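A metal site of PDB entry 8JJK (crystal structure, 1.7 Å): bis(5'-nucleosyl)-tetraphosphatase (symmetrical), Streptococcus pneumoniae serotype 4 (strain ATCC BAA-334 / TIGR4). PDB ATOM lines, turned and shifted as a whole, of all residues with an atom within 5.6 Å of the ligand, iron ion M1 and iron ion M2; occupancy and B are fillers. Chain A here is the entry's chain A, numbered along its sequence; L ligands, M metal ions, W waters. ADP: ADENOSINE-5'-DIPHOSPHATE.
N6 of the ligand sits close to O of Tyr 180.
O3B of the ligand lies close to NH2 of Arg 141 (2.9 Å).
N6 of the ligand sits at hydrogen-bond distance from OG1 of Thr 183 (2.7 Å).
The side-chain amide nitrogen (ND2) of Asn 88 sits at hydrogen-bond distance from a nitrogen (N3) of the ligand, at 3.4 Å.
The side-chain hydroxyl (OG1) of Thr 118 lies close to an oxygen (O2A) of the ligand, 2.8 Å away.
NH1 of Arg 26 is in salt-bridge range of O1B of the ligand (3.6 Å).
O1B of the ligand is in salt-bridge range of NZ of Lys 62 (3.2 Å).
N of Tyr 180 lies within hydrogen-bond range of N1 of the ligand, at 3.0 Å.
Iron ion M1 is bound by water W8 (2.0 Å).
OD1 of Asp 59 binds iron ion M1.
Iron ion M1 is bound by O2B of the ligand, at 2.1 Å.
O2A of the ligand is bound to iron ion M1 (2.1 Å).
A ring nitrogen (NE2) of His 117 is bound to iron ion M1 (2.2 Å).
A ring nitrogen (NE2) of His 91 is bound to iron ion M1 (2.2 Å).
Residues that only touch iron ion M1: Thr 118.
Four residues have an atom within 4 Å of iron ion M1: Asp 59, His 91, His 117 and Thr 118.
The nearest printed residue that does not touch iron ion M1 is His 58 (4.1 Å).
Residues that only touch iron ion M2: Arg 141 (3.9 Å) and Arg 26 (3.9 Å).
Within 4 Å of iron ion M2: Arg 26, His 29, His 58, Asp 59, Asp 135 and Arg 141.
Iron ion M2 is bound by water W8 (2.0 Å).
A ring nitrogen (NE2) of His 29 binds iron ion M2.
Iron ion M2 is bound by the side-chain carboxylate (OD1) of Asp 135, at 2.1 Å.
O3B of the ligand is bound to iron ion M2 (2.2 Å).
NE2 of His 58 is bound to iron ion M2 (2.2 Å).
OD2 of Asp 59 is bound to iron ion M2, at 2.2 Å.
OD2 of Asp 135 lies within salt-bridge range of NH2 of Arg 141.
The backbone carbonyl oxygen (O) of Asn 88 is in hydrogen-bond range of a ring nitrogen (ND1) of His 91, at 3.2 Å.
OD2 of Asp 59 sits close to NH1 of Arg 26, at 3.0 Å.
The side-chain hydroxyl (OG1) of Thr 168 sits at hydrogen-bond distance from the backbone carbonyl oxygen (O) of Glu 164 (2.9 Å).
NE2 of His 117 lies close to OG1 of Thr 118 (3.2 Å).
Water W8 lies within hydrogen-bond range of the side-chain carboxylate of Asp 135 (2.6 Å) and an oxygen (O3A) of the ligand (2.9 Å).
Water W2 lies within hydrogen-bond range of N7 of the ligand, O of Thr 118 and OG1 of Thr 183.
Water W1 lies within hydrogen-bond range of an oxygen (O1B) of the ligand (2.7 Å), the guanidinium group of Arg 26 (3.4 Å) and the guanidinium group of Arg 141 (3.4 Å).
Water W5 lies within hydrogen-bond range of the side-chain carboxylate (OD2) of Asp 135 (3.1 Å), the guanidinium group (NH2) of Arg 141 (3.2 Å) and an oxygen (O1A) of the ligand (3.2 Å).
Water W4 lies within hydrogen-bond range of O3' of the ligand (3.3 Å) and ND2 of Asn 88 (3.4 Å).
Merely in contact with the ligand: Pro 178, Leu 172, Thr 168 and Ile 179.
Hydrophobic or aromatic side chains that line the ligand: His 29, His 91, His 117, Leu 172, Ile 179 and Tyr 180.
16 residues have an atom within 4 Å of the ligand: Arg 26, His 29, Asp 59, Lys 62, Asn 88, His 91, His 117, Thr 118, Asp 135, Arg 141, Thr 168, Leu 172, Pro 178, Ile 179, Tyr 180 and Thr 183.
The nearest printed residue that does not touch the ligand is Val 119 (4.3 Å).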
ATOM      1  N   ARG A  26      32.396  36.710   1.216  1.00  0.00           N
ATOM      2  CA  ARG A  26      31.422  35.885   0.520  1.00  0.00           C
ATOM      3  C   ARG A  26      31.581  35.984  -1.008  1.00  0.00           C
ATOM      4  O   ARG A  26      31.483  34.976  -1.702  1.00  0.00           O
ATOM      5  CB  ARG A  26      29.994  36.224   0.970  1.00  0.00           C
ATOM      6  CG  ARG A  26      28.901  35.334   0.378  1.00  0.00           C
ATOM      7  CD  ARG A  26      29.116  33.855   0.664  1.00  0.00           C
ATOM      8  NE  ARG A  26      29.234  33.603   2.099  1.00  0.00           N
ATOM      9  CZ  ARG A  26      29.494  32.410   2.639  1.00  0.00           C
ATOM     10  NH1 ARG A  26      29.646  31.336   1.871  1.00  0.00           N
ATOM     11  NH2 ARG A  26      29.589  32.285   3.955  1.00  0.00           N
ATOM     12  N   HIS A  29      34.573  34.048  -2.028  1.00  0.00           N
ATOM     13  CA  HIS A  29      34.166  32.638  -2.036  1.00  0.00           C
ATOM     14  C   HIS A  29      33.458  32.285  -3.338  1.00  0.00           C
ATOM     15  O   HIS A  29      33.758  31.258  -3.958  1.00  0.00           O
ATOM     16  CB  HIS A  29      33.277  32.337  -0.826  1.00  0.00           C
ATOM     17  CG  HIS A  29      32.501  31.058  -0.921  1.00  0.00           C
ATOM     18  ND1 HIS A  29      33.107  29.816  -0.888  1.00  0.00           N
ATOM     19  CD2 HIS A  29      31.170  30.818  -1.026  1.00  0.00           C
ATOM     20  CE1 HIS A  29      32.179  28.875  -0.962  1.00  0.00           C
ATOM     21  NE2 HIS A  29      31.001  29.461  -1.035  1.00  0.00           N
ATOM     22  N   VAL A  33      34.410  29.550  -6.131  1.00  0.00           N
ATOM     23  CA  VAL A  33      33.536  28.460  -6.605  1.00  0.00           C
ATOM     24  C   VAL A  33      33.389  28.513  -8.131  1.00  0.00           C
ATOM     25  O   VAL A  33      33.352  27.484  -8.785  1.00  0.00           O
ATOM     26  CB  VAL A  33      32.165  28.464  -5.874  1.00  0.00           C
ATOM     27  CG1 VAL A  33      31.256  27.348  -6.365  1.00  0.00           C
ATOM     28  CG2 VAL A  33      32.385  28.338  -4.374  1.00  0.00           C
ATOM     29  N   HIS A  58      25.939  30.682  -6.793  1.00  0.00           N
ATOM     30  CA  HIS A  58      25.330  29.703  -5.891  1.00  0.00           C
ATOM     31  C   HIS A  58      24.910  30.329  -4.540  1.00  0.00           C
ATOM     32  O   HIS A  58      23.884  29.955  -3.982  1.00  0.00           O
ATOM     33  CB  HIS A  58      26.239  28.475  -5.702  1.00  0.00           C
ATOM     34  CG  HIS A  58      27.339  28.707  -4.728  1.00  0.00           C
ATOM     35  ND1 HIS A  58      28.413  29.524  -4.996  1.00  0.00           N
ATOM     36  CD2 HIS A  58      27.507  28.272  -3.461  1.00  0.00           C
ATOM     37  CE1 HIS A  58      29.203  29.573  -3.934  1.00  0.00           C
ATOM     38  NE2 HIS A  58      28.678  28.808  -2.993  1.00  0.00           N
ATOM     39  N   ASP A  59      25.704  31.289  -4.057  1.00  0.00           N
ATOM     40  CA  ASP A  59      25.472  31.949  -2.762  1.00  0.00           C
ATOM     41  C   ASP A  59      24.937  33.373  -2.916  1.00  0.00           C
ATOM     42  O   ASP A  59      25.029  34.180  -1.975  1.00  0.00           O
ATOM     43  CB  ASP A  59      26.742  31.946  -1.896  1.00  0.00           C
ATOM     44  CG  ASP A  59      26.900  30.675  -1.044  1.00  0.00           C
ATOM     45  OD1 ASP A  59      25.934  29.886  -0.894  1.00  0.00           O
ATOM     46  OD2 ASP A  59      28.013  30.480  -0.519  1.00  0.00           O
ATOM     47  N   LYS A  62      22.645  34.579  -0.142  1.00  0.00           N
ATOM     48  CA  LYS A  62      23.140  34.274   1.203  1.00  0.00           C
ATOM     49  C   LYS A  62      22.694  35.283   2.267  1.00  0.00           C
ATOM     50  O   LYS A  62      22.458  34.903   3.415  1.00  0.00           O
ATOM     51  CB  LYS A  62      24.674  34.155   1.201  1.00  0.00           C
ATOM     52  CG  LYS A  62      25.308  33.615   2.483  1.00  0.00           C
ATOM     53  CD  LYS A  62      25.071  32.118   2.698  1.00  0.00           C
ATOM     54  CE  LYS A  62      25.894  31.632   3.892  1.00  0.00           C
ATOM     55  NZ  LYS A  62      25.858  30.156   4.100  1.00  0.00           N
ATOM     56  N   TRP A  85      12.690  25.941   9.004  1.00  0.00           N
ATOM     57  CA  TRP A  85      14.146  25.943   8.907  1.00  0.00           C
ATOM     58  C   TRP A  85      14.686  27.372   8.862  1.00  0.00           C
ATOM     59  O   TRP A  85      14.086  28.269   9.465  1.00  0.00           O
ATOM     60  CB  TRP A  85      14.569  25.070   7.720  1.00  0.00           C
ATOM     61  CG  TRP A  85      14.038  23.687   7.905  1.00  0.00           C
ATOM     62  CD1 TRP A  85      12.789  23.225   7.545  1.00  0.00           C
ATOM     63  CD2 TRP A  85      14.674  22.606   8.567  1.00  0.00           C
ATOM     64  NE1 TRP A  85      12.634  21.921   7.929  1.00  0.00           N
ATOM     65  CE2 TRP A  85      13.776  21.514   8.555  1.00  0.00           C
ATOM     66  CE3 TRP A  85      15.942  22.444   9.155  1.00  0.00           C
ATOM     67  CZ2 TRP A  85      14.103  20.265   9.105  1.00  0.00           C
ATOM     68  CZ3 TRP A  85      16.270  21.204   9.702  1.00  0.00           C
ATOM     69  CH2 TRP A  85      15.348  20.136   9.690  1.00  0.00           C
ATOM     70  N   ASN A  88      20.416  28.471   6.163  1.00  0.00           N
ATOM     71  CA  ASN A  88      21.186  27.333   5.624  1.00  0.00           C
ATOM     72  C   ASN A  88      20.428  26.605   4.531  1.00  0.00           C
ATOM     73  O   ASN A  88      20.968  26.371   3.444  1.00  0.00           O
ATOM     74  CB  ASN A  88      21.572  26.327   6.721  1.00  0.00           C
ATOM     75  CG  ASN A  88      22.611  26.850   7.674  1.00  0.00           C
ATOM     76  OD1 ASN A  88      23.218  27.909   7.460  1.00  0.00           O
ATOM     77  ND2 ASN A  88      22.843  26.098   8.744  1.00  0.00           N
ATOM     78  N   VAL A  89      19.171  26.250   4.820  1.00  0.00           N
ATOM     79  CA  VAL A  89      18.304  25.606   3.851  1.00  0.00           C
ATOM     80  C   VAL A  89      17.829  26.619   2.804  1.00  0.00           C
ATOM     81  O   VAL A  89      17.854  26.322   1.599  1.00  0.00           O
ATOM     82  CB  VAL A  89      17.102  24.895   4.526  1.00  0.00           C
ATOM     83  CG1 VAL A  89      16.147  24.311   3.498  1.00  0.00           C
ATOM     84  CG2 VAL A  89      17.573  23.789   5.481  1.00  0.00           C
ATOM     85  N   HIS A  91      18.830  29.633   1.502  1.00  0.00           N
ATOM     86  CA  HIS A  91      19.563  30.509   0.564  1.00  0.00           C
ATOM     87  C   HIS A  91      19.721  29.857  -0.809  1.00  0.00           C
ATOM     88  O   HIS A  91      19.734  30.542  -1.823  1.00  0.00           O
ATOM     89  CB  HIS A  91      20.862  31.065   1.160  1.00  0.00           C
ATOM     90  CG  HIS A  91      21.977  30.063   1.238  1.00  0.00           C
ATOM     91  ND1 HIS A  91      22.051  29.122   2.233  1.00  0.00           N
ATOM     92  CD2 HIS A  91      23.080  29.898   0.474  1.00  0.00           C
ATOM     93  CE1 HIS A  91      23.143  28.390   2.066  1.00  0.00           C
ATOM     94  NE2 HIS A  91      23.781  28.845   1.010  1.00  0.00           N
ATOM     95  N   HIS A 117      22.576  23.101  -3.771  1.00  0.00           N
ATOM     96  CA  HIS A 117      24.034  23.170  -3.524  1.00  0.00           C
ATOM     97  C   HIS A 117      24.414  22.936  -2.063  1.00  0.00           C
ATOM     98  O   HIS A 117      25.550  22.556  -1.767  1.00  0.00           O
ATOM     99  CB  HIS A 117      24.638  24.479  -4.024  1.00  0.00           C
ATOM    100  CG  HIS A 117      24.492  25.612  -3.062  1.00  0.00           C
ATOM    101  ND1 HIS A 117      23.472  26.529  -3.139  1.00  0.00           N
ATOM    102  CD2 HIS A 117      25.233  25.979  -1.980  1.00  0.00           C
ATOM    103  CE1 HIS A 117      23.585  27.413  -2.162  1.00  0.00           C
ATOM    104  NE2 HIS A 117      24.654  27.096  -1.445  1.00  0.00           N
ATOM    105  N   THR A 118      23.469  23.159  -1.149  1.00  0.00           N
ATOM    106  CA  THR A 118      23.708  22.947   0.280  1.00  0.00           C
ATOM    107  C   THR A 118      23.353  21.522   0.717  1.00  0.00           C
ATOM    108  O   THR A 118      24.145  20.853   1.387  1.00  0.00           O
ATOM    109  CB  THR A 118      22.889  23.945   1.125  1.00  0.00           C
ATOM    110  OG1 THR A 118      23.136  25.279   0.677  1.00  0.00           O
ATOM    111  CG2 THR A 118      23.212  23.817   2.618  1.00  0.00           C
ATOM    112  N   VAL A 119      22.164  21.080   0.341  1.00  0.00           N
ATOM    113  CA  VAL A 119      21.597  19.832   0.869  1.00  0.00           C
ATOM    114  C   VAL A 119      21.705  18.636  -0.071  1.00  0.00           C
ATOM    115  O   VAL A 119      21.489  17.492   0.342  1.00  0.00           O
ATOM    116  CB  VAL A 119      20.110  20.030   1.282  1.00  0.00           C
ATOM    117  CG1 VAL A 119      20.000  21.072   2.400  1.00  0.00           C
ATOM    118  CG2 VAL A 119      19.252  20.432   0.085  1.00  0.00           C
ATOM    119  N   ASP A 135      31.825  24.082  -4.175  1.00  0.00           N
ATOM    120  CA  ASP A 135      31.519  24.909  -3.018  1.00  0.00           C
ATOM    121  C   ASP A 135      32.434  24.540  -1.832  1.00  0.00           C
ATOM    122  O   ASP A 135      32.897  25.413  -1.063  1.00  0.00           O
ATOM    123  CB  ASP A 135      30.045  24.686  -2.645  1.00  0.00           C
ATOM    124  CG  ASP A 135      29.557  25.586  -1.539  1.00  0.00           C
ATOM    125  OD1 ASP A 135      30.085  26.711  -1.351  1.00  0.00           O
ATOM    126  OD2 ASP A 135      28.589  25.152  -0.876  1.00  0.00           O
ATOM    127  N   ARG A 141      38.801  28.000   0.874  1.00  0.00           N
ATOM    128  CA  ARG A 141      38.416  27.142   2.013  1.00  0.00           C
ATOM    129  C   ARG A 141      39.662  26.570   2.683  1.00  0.00           C
ATOM    130  O   ARG A 141      40.625  26.212   1.999  1.00  0.00           O
ATOM    131  CB  ARG A 141      37.480  26.022   1.558  1.00  0.00           C
ATOM    132  CG  ARG A 141      36.090  26.470   1.105  1.00  0.00           C
ATOM    133  CD  ARG A 141      35.089  26.482   2.257  1.00  0.00           C
ATOM    134  NE  ARG A 141      33.756  26.177   1.758  1.00  0.00           N
ATOM    135  CZ  ARG A 141      32.659  26.902   1.963  1.00  0.00           C
ATOM    136  NH1 ARG A 141      32.695  28.010   2.724  1.00  0.00           N
ATOM    137  NH2 ARG A 141      31.515  26.510   1.429  1.00  0.00           N
ATOM    138  N   GLU A 164      31.950  14.737   1.155  1.00  0.00           N
ATOM    139  CA  GLU A 164      31.404  16.002   1.662  1.00  0.00           C
ATOM    140  C   GLU A 164      30.150  15.777   2.496  1.00  0.00           C
ATOM    141  O   GLU A 164      29.987  16.374   3.578  1.00  0.00           O
ATOM    142  CB  GLU A 164      31.118  16.980   0.520  1.00  0.00           C
ATOM    143  CG  GLU A 164      30.457  18.260   1.010  1.00  0.00           C
ATOM    144  CD  GLU A 164      30.125  19.272  -0.086  1.00  0.00           C
ATOM    145  OE1 GLU A 164      30.561  19.084  -1.246  1.00  0.00           O
ATOM    146  OE2 GLU A 164      29.430  20.253   0.224  1.00  0.00           O
ATOM    147  N   THR A 168      29.565  16.484   6.488  1.00  0.00           N
ATOM    148  CA  THR A 168      28.554  17.447   6.891  1.00  0.00           C
ATOM    149  C   THR A 168      27.575  16.863   7.897  1.00  0.00           C
ATOM    150  O   THR A 168      27.278  17.515   8.922  1.00  0.00           O
ATOM    151  CB  THR A 168      27.869  18.026   5.663  1.00  0.00           C
ATOM    152  OG1 THR A 168      28.870  18.739   4.922  1.00  0.00           O
ATOM    153  CG2 THR A 168      26.731  18.976   6.057  1.00  0.00           C
ATOM    154  N   LEU A 172      27.332  18.264  11.675  1.00  0.00           N
ATOM    155  CA  LEU A 172      26.056  18.778  12.216  1.00  0.00           C
ATOM    156  C   LEU A 172      25.673  18.042  13.493  1.00  0.00           C
ATOM    157  O   LEU A 172      25.284  18.667  14.485  1.00  0.00           O
ATOM    158  CB  LEU A 172      24.956  18.737  11.154  1.00  0.00           C
ATOM    159  CG  LEU A 172      25.147  19.711   9.985  1.00  0.00           C
ATOM    160  CD1 LEU A 172      24.084  19.403   8.943  1.00  0.00           C
ATOM    161  CD2 LEU A 172      25.087  21.173  10.401  1.00  0.00           C
ATOM    162  N   PRO A 178      20.071  20.764  13.958  1.00  0.00           N
ATOM    163  CA  PRO A 178      19.091  20.018  13.162  1.00  0.00           C
ATOM    164  C   PRO A 178      19.631  19.744  11.768  1.00  0.00           C
ATOM    165  O   PRO A 178      20.391  20.571  11.218  1.00  0.00           O
ATOM    166  CB  PRO A 178      17.894  20.971  13.079  1.00  0.00           C
ATOM    167  CG  PRO A 178      18.055  21.933  14.200  1.00  0.00           C
ATOM    168  CD  PRO A 178      19.525  22.029  14.490  1.00  0.00           C
ATOM    169  N   ILE A 179      19.266  18.587  11.204  1.00  0.00           N
ATOM    170  CA  ILE A 179      19.720  18.158   9.887  1.00  0.00           C
ATOM    171  C   ILE A 179      18.510  18.102   8.946  1.00  0.00           C
ATOM    172  O   ILE A 179      17.601  17.305   9.141  1.00  0.00           O
ATOM    173  CB  ILE A 179      20.449  16.793   9.941  1.00  0.00           C
ATOM    174  CG1 ILE A 179      21.706  16.932  10.807  1.00  0.00           C
ATOM    175  CG2 ILE A 179      20.786  16.282   8.532  1.00  0.00           C
ATOM    176  CD1 ILE A 179      22.306  15.623  11.279  1.00  0.00           C
ATOM    177  N   TYR A 180      18.523  18.959   7.924  1.00  0.00           N
ATOM    178  CA  TYR A 180      17.437  18.972   6.941  1.00  0.00           C
ATOM    179  C   TYR A 180      17.344  17.599   6.286  1.00  0.00           C
ATOM    180  O   TYR A 180      18.363  17.037   5.882  1.00  0.00           O
ATOM    181  CB  TYR A 180      17.660  20.089   5.914  1.00  0.00           C
ATOM    182  CG  TYR A 180      16.472  20.300   5.018  1.00  0.00           C
ATOM    183  CD1 TYR A 180      15.299  20.852   5.519  1.00  0.00           C
ATOM    184  CD2 TYR A 180      16.524  19.951   3.669  1.00  0.00           C
ATOM    185  CE1 TYR A 180      14.186  21.046   4.704  1.00  0.00           C
ATOM    186  CE2 TYR A 180      15.417  20.159   2.838  1.00  0.00           C
ATOM    187  CZ  TYR A 180      14.257  20.708   3.359  1.00  0.00           C
ATOM    188  OH  TYR A 180      13.180  20.897   2.540  1.00  0.00           O
ATOM    189  N   PRO A 181      16.144  16.998   6.257  1.00  0.00           N
ATOM    190  CA  PRO A 181      16.057  15.601   5.834  1.00  0.00           C
ATOM    191  C   PRO A 181      16.582  15.312   4.427  1.00  0.00           C
ATOM    192  O   PRO A 181      17.077  14.210   4.194  1.00  0.00           O
ATOM    193  CB  PRO A 181      14.566  15.284   5.976  1.00  0.00           C
ATOM    194  CG  PRO A 181      14.183  16.117   7.153  1.00  0.00           C
ATOM    195  CD  PRO A 181      14.887  17.430   6.894  1.00  0.00           C
ATOM    196  N   THR A 183      19.259  16.252   3.135  1.00  0.00           N
ATOM    197  CA  THR A 183      20.665  15.886   3.293  1.00  0.00           C
ATOM    198  C   THR A 183      20.861  14.397   3.550  1.00  0.00           C
ATOM    199  O   THR A 183      21.809  13.799   3.043  1.00  0.00           O
ATOM    200  CB  THR A 183      21.328  16.740   4.376  1.00  0.00           C
ATOM    201  OG1 THR A 183      21.444  18.065   3.878  1.00  0.00           O
ATOM    202  CG2 THR A 183      22.726  16.246   4.747  1.00  0.00           C
HETATM  203  PB  ADP L   1      28.149  28.165   2.260  1.00  0.00           P
HETATM  204  O1B ADP L   1      28.527  28.453   3.695  1.00  0.00           O
HETATM  205  O2B ADP L   1      26.843  28.819   1.800  1.00  0.00           O
HETATM  206  O3B ADP L   1      29.324  28.452   1.345  1.00  0.00           O
HETATM  207  PA  ADP L   1      26.644  25.635   2.177  1.00  0.00           P
HETATM  208  O1A ADP L   1      27.016  24.252   1.711  1.00  0.00           O
HETATM  209  O2A ADP L   1      25.547  26.368   1.458  1.00  0.00           O
HETATM  210  O3A ADP L   1      27.986  26.542   2.268  1.00  0.00           O
HETATM  211  O5' ADP L   1      26.272  25.478   3.723  1.00  0.00           O
HETATM  212  C5' ADP L   1      25.737  26.534   4.514  1.00  0.00           C
HETATM  213  C4' ADP L   1      25.596  25.972   5.928  1.00  0.00           C
HETATM  214  O4' ADP L   1      24.520  25.037   5.911  1.00  0.00           O
HETATM  215  C3' ADP L   1      26.834  25.223   6.459  1.00  0.00           C
HETATM  216  O3' ADP L   1      27.137  25.709   7.776  1.00  0.00           O
HETATM  217  C2' ADP L   1      26.412  23.757   6.494  1.00  0.00           C
HETATM  218  O2' ADP L   1      26.968  22.972   7.561  1.00  0.00           O
HETATM  219  C1' ADP L   1      24.900  23.878   6.664  1.00  0.00           C
HETATM  220  N9  ADP L   1      24.148  22.663   6.285  1.00  0.00           N
HETATM  221  C8  ADP L   1      24.465  21.759   5.338  1.00  0.00           C
HETATM  222  N7  ADP L   1      23.538  20.778   5.271  1.00  0.00           N
HETATM  223  C5  ADP L   1      22.630  21.063   6.211  1.00  0.00           C
HETATM  224  C6  ADP L   1      21.393  20.452   6.725  1.00  0.00           C
HETATM  225  N6  ADP L   1      20.946  19.327   6.190  1.00  0.00           N
HETATM  226  N1  ADP L   1      20.723  21.056   7.732  1.00  0.00           N
HETATM  227  C2  ADP L   1      21.176  22.195   8.276  1.00  0.00           C
HETATM  228  N3  ADP L   1      22.290  22.835   7.880  1.00  0.00           N
HETATM  229  C4  ADP L   1      23.030  22.301   6.876  1.00  0.00           C
HETATM  230 FE    FE M   1      25.677  28.103   0.196  1.00  0.00          FE
HETATM  231 FE    FE M   2      29.090  28.532  -0.843  1.00  0.00          FE
HETATM  232 MG    MG M   3      27.893  22.403  -0.563  1.00  0.00          MG
HETATM  233  O   HOH W   1      30.644  29.298   5.048  1.00  0.00           O
HETATM  234  O   HOH W   2      24.015  19.073   3.482  1.00  0.00           O
HETATM  235  O   HOH W   3      29.721  26.293   4.848  1.00  0.00           O
HETATM  236  O   HOH W   4      25.530  24.967  10.552  1.00  0.00           O
HETATM  237  O   HOH W   5      30.170  23.602   1.312  1.00  0.00           O
HETATM  238  O   HOH W   6      20.736  23.179  11.242  1.00  0.00           O
HETATM  239  O   HOH W   7      27.040  22.304   3.283  1.00  0.00           O
HETATM  240  O   HOH W   8      27.485  27.472  -0.449  1.00  0.00           O
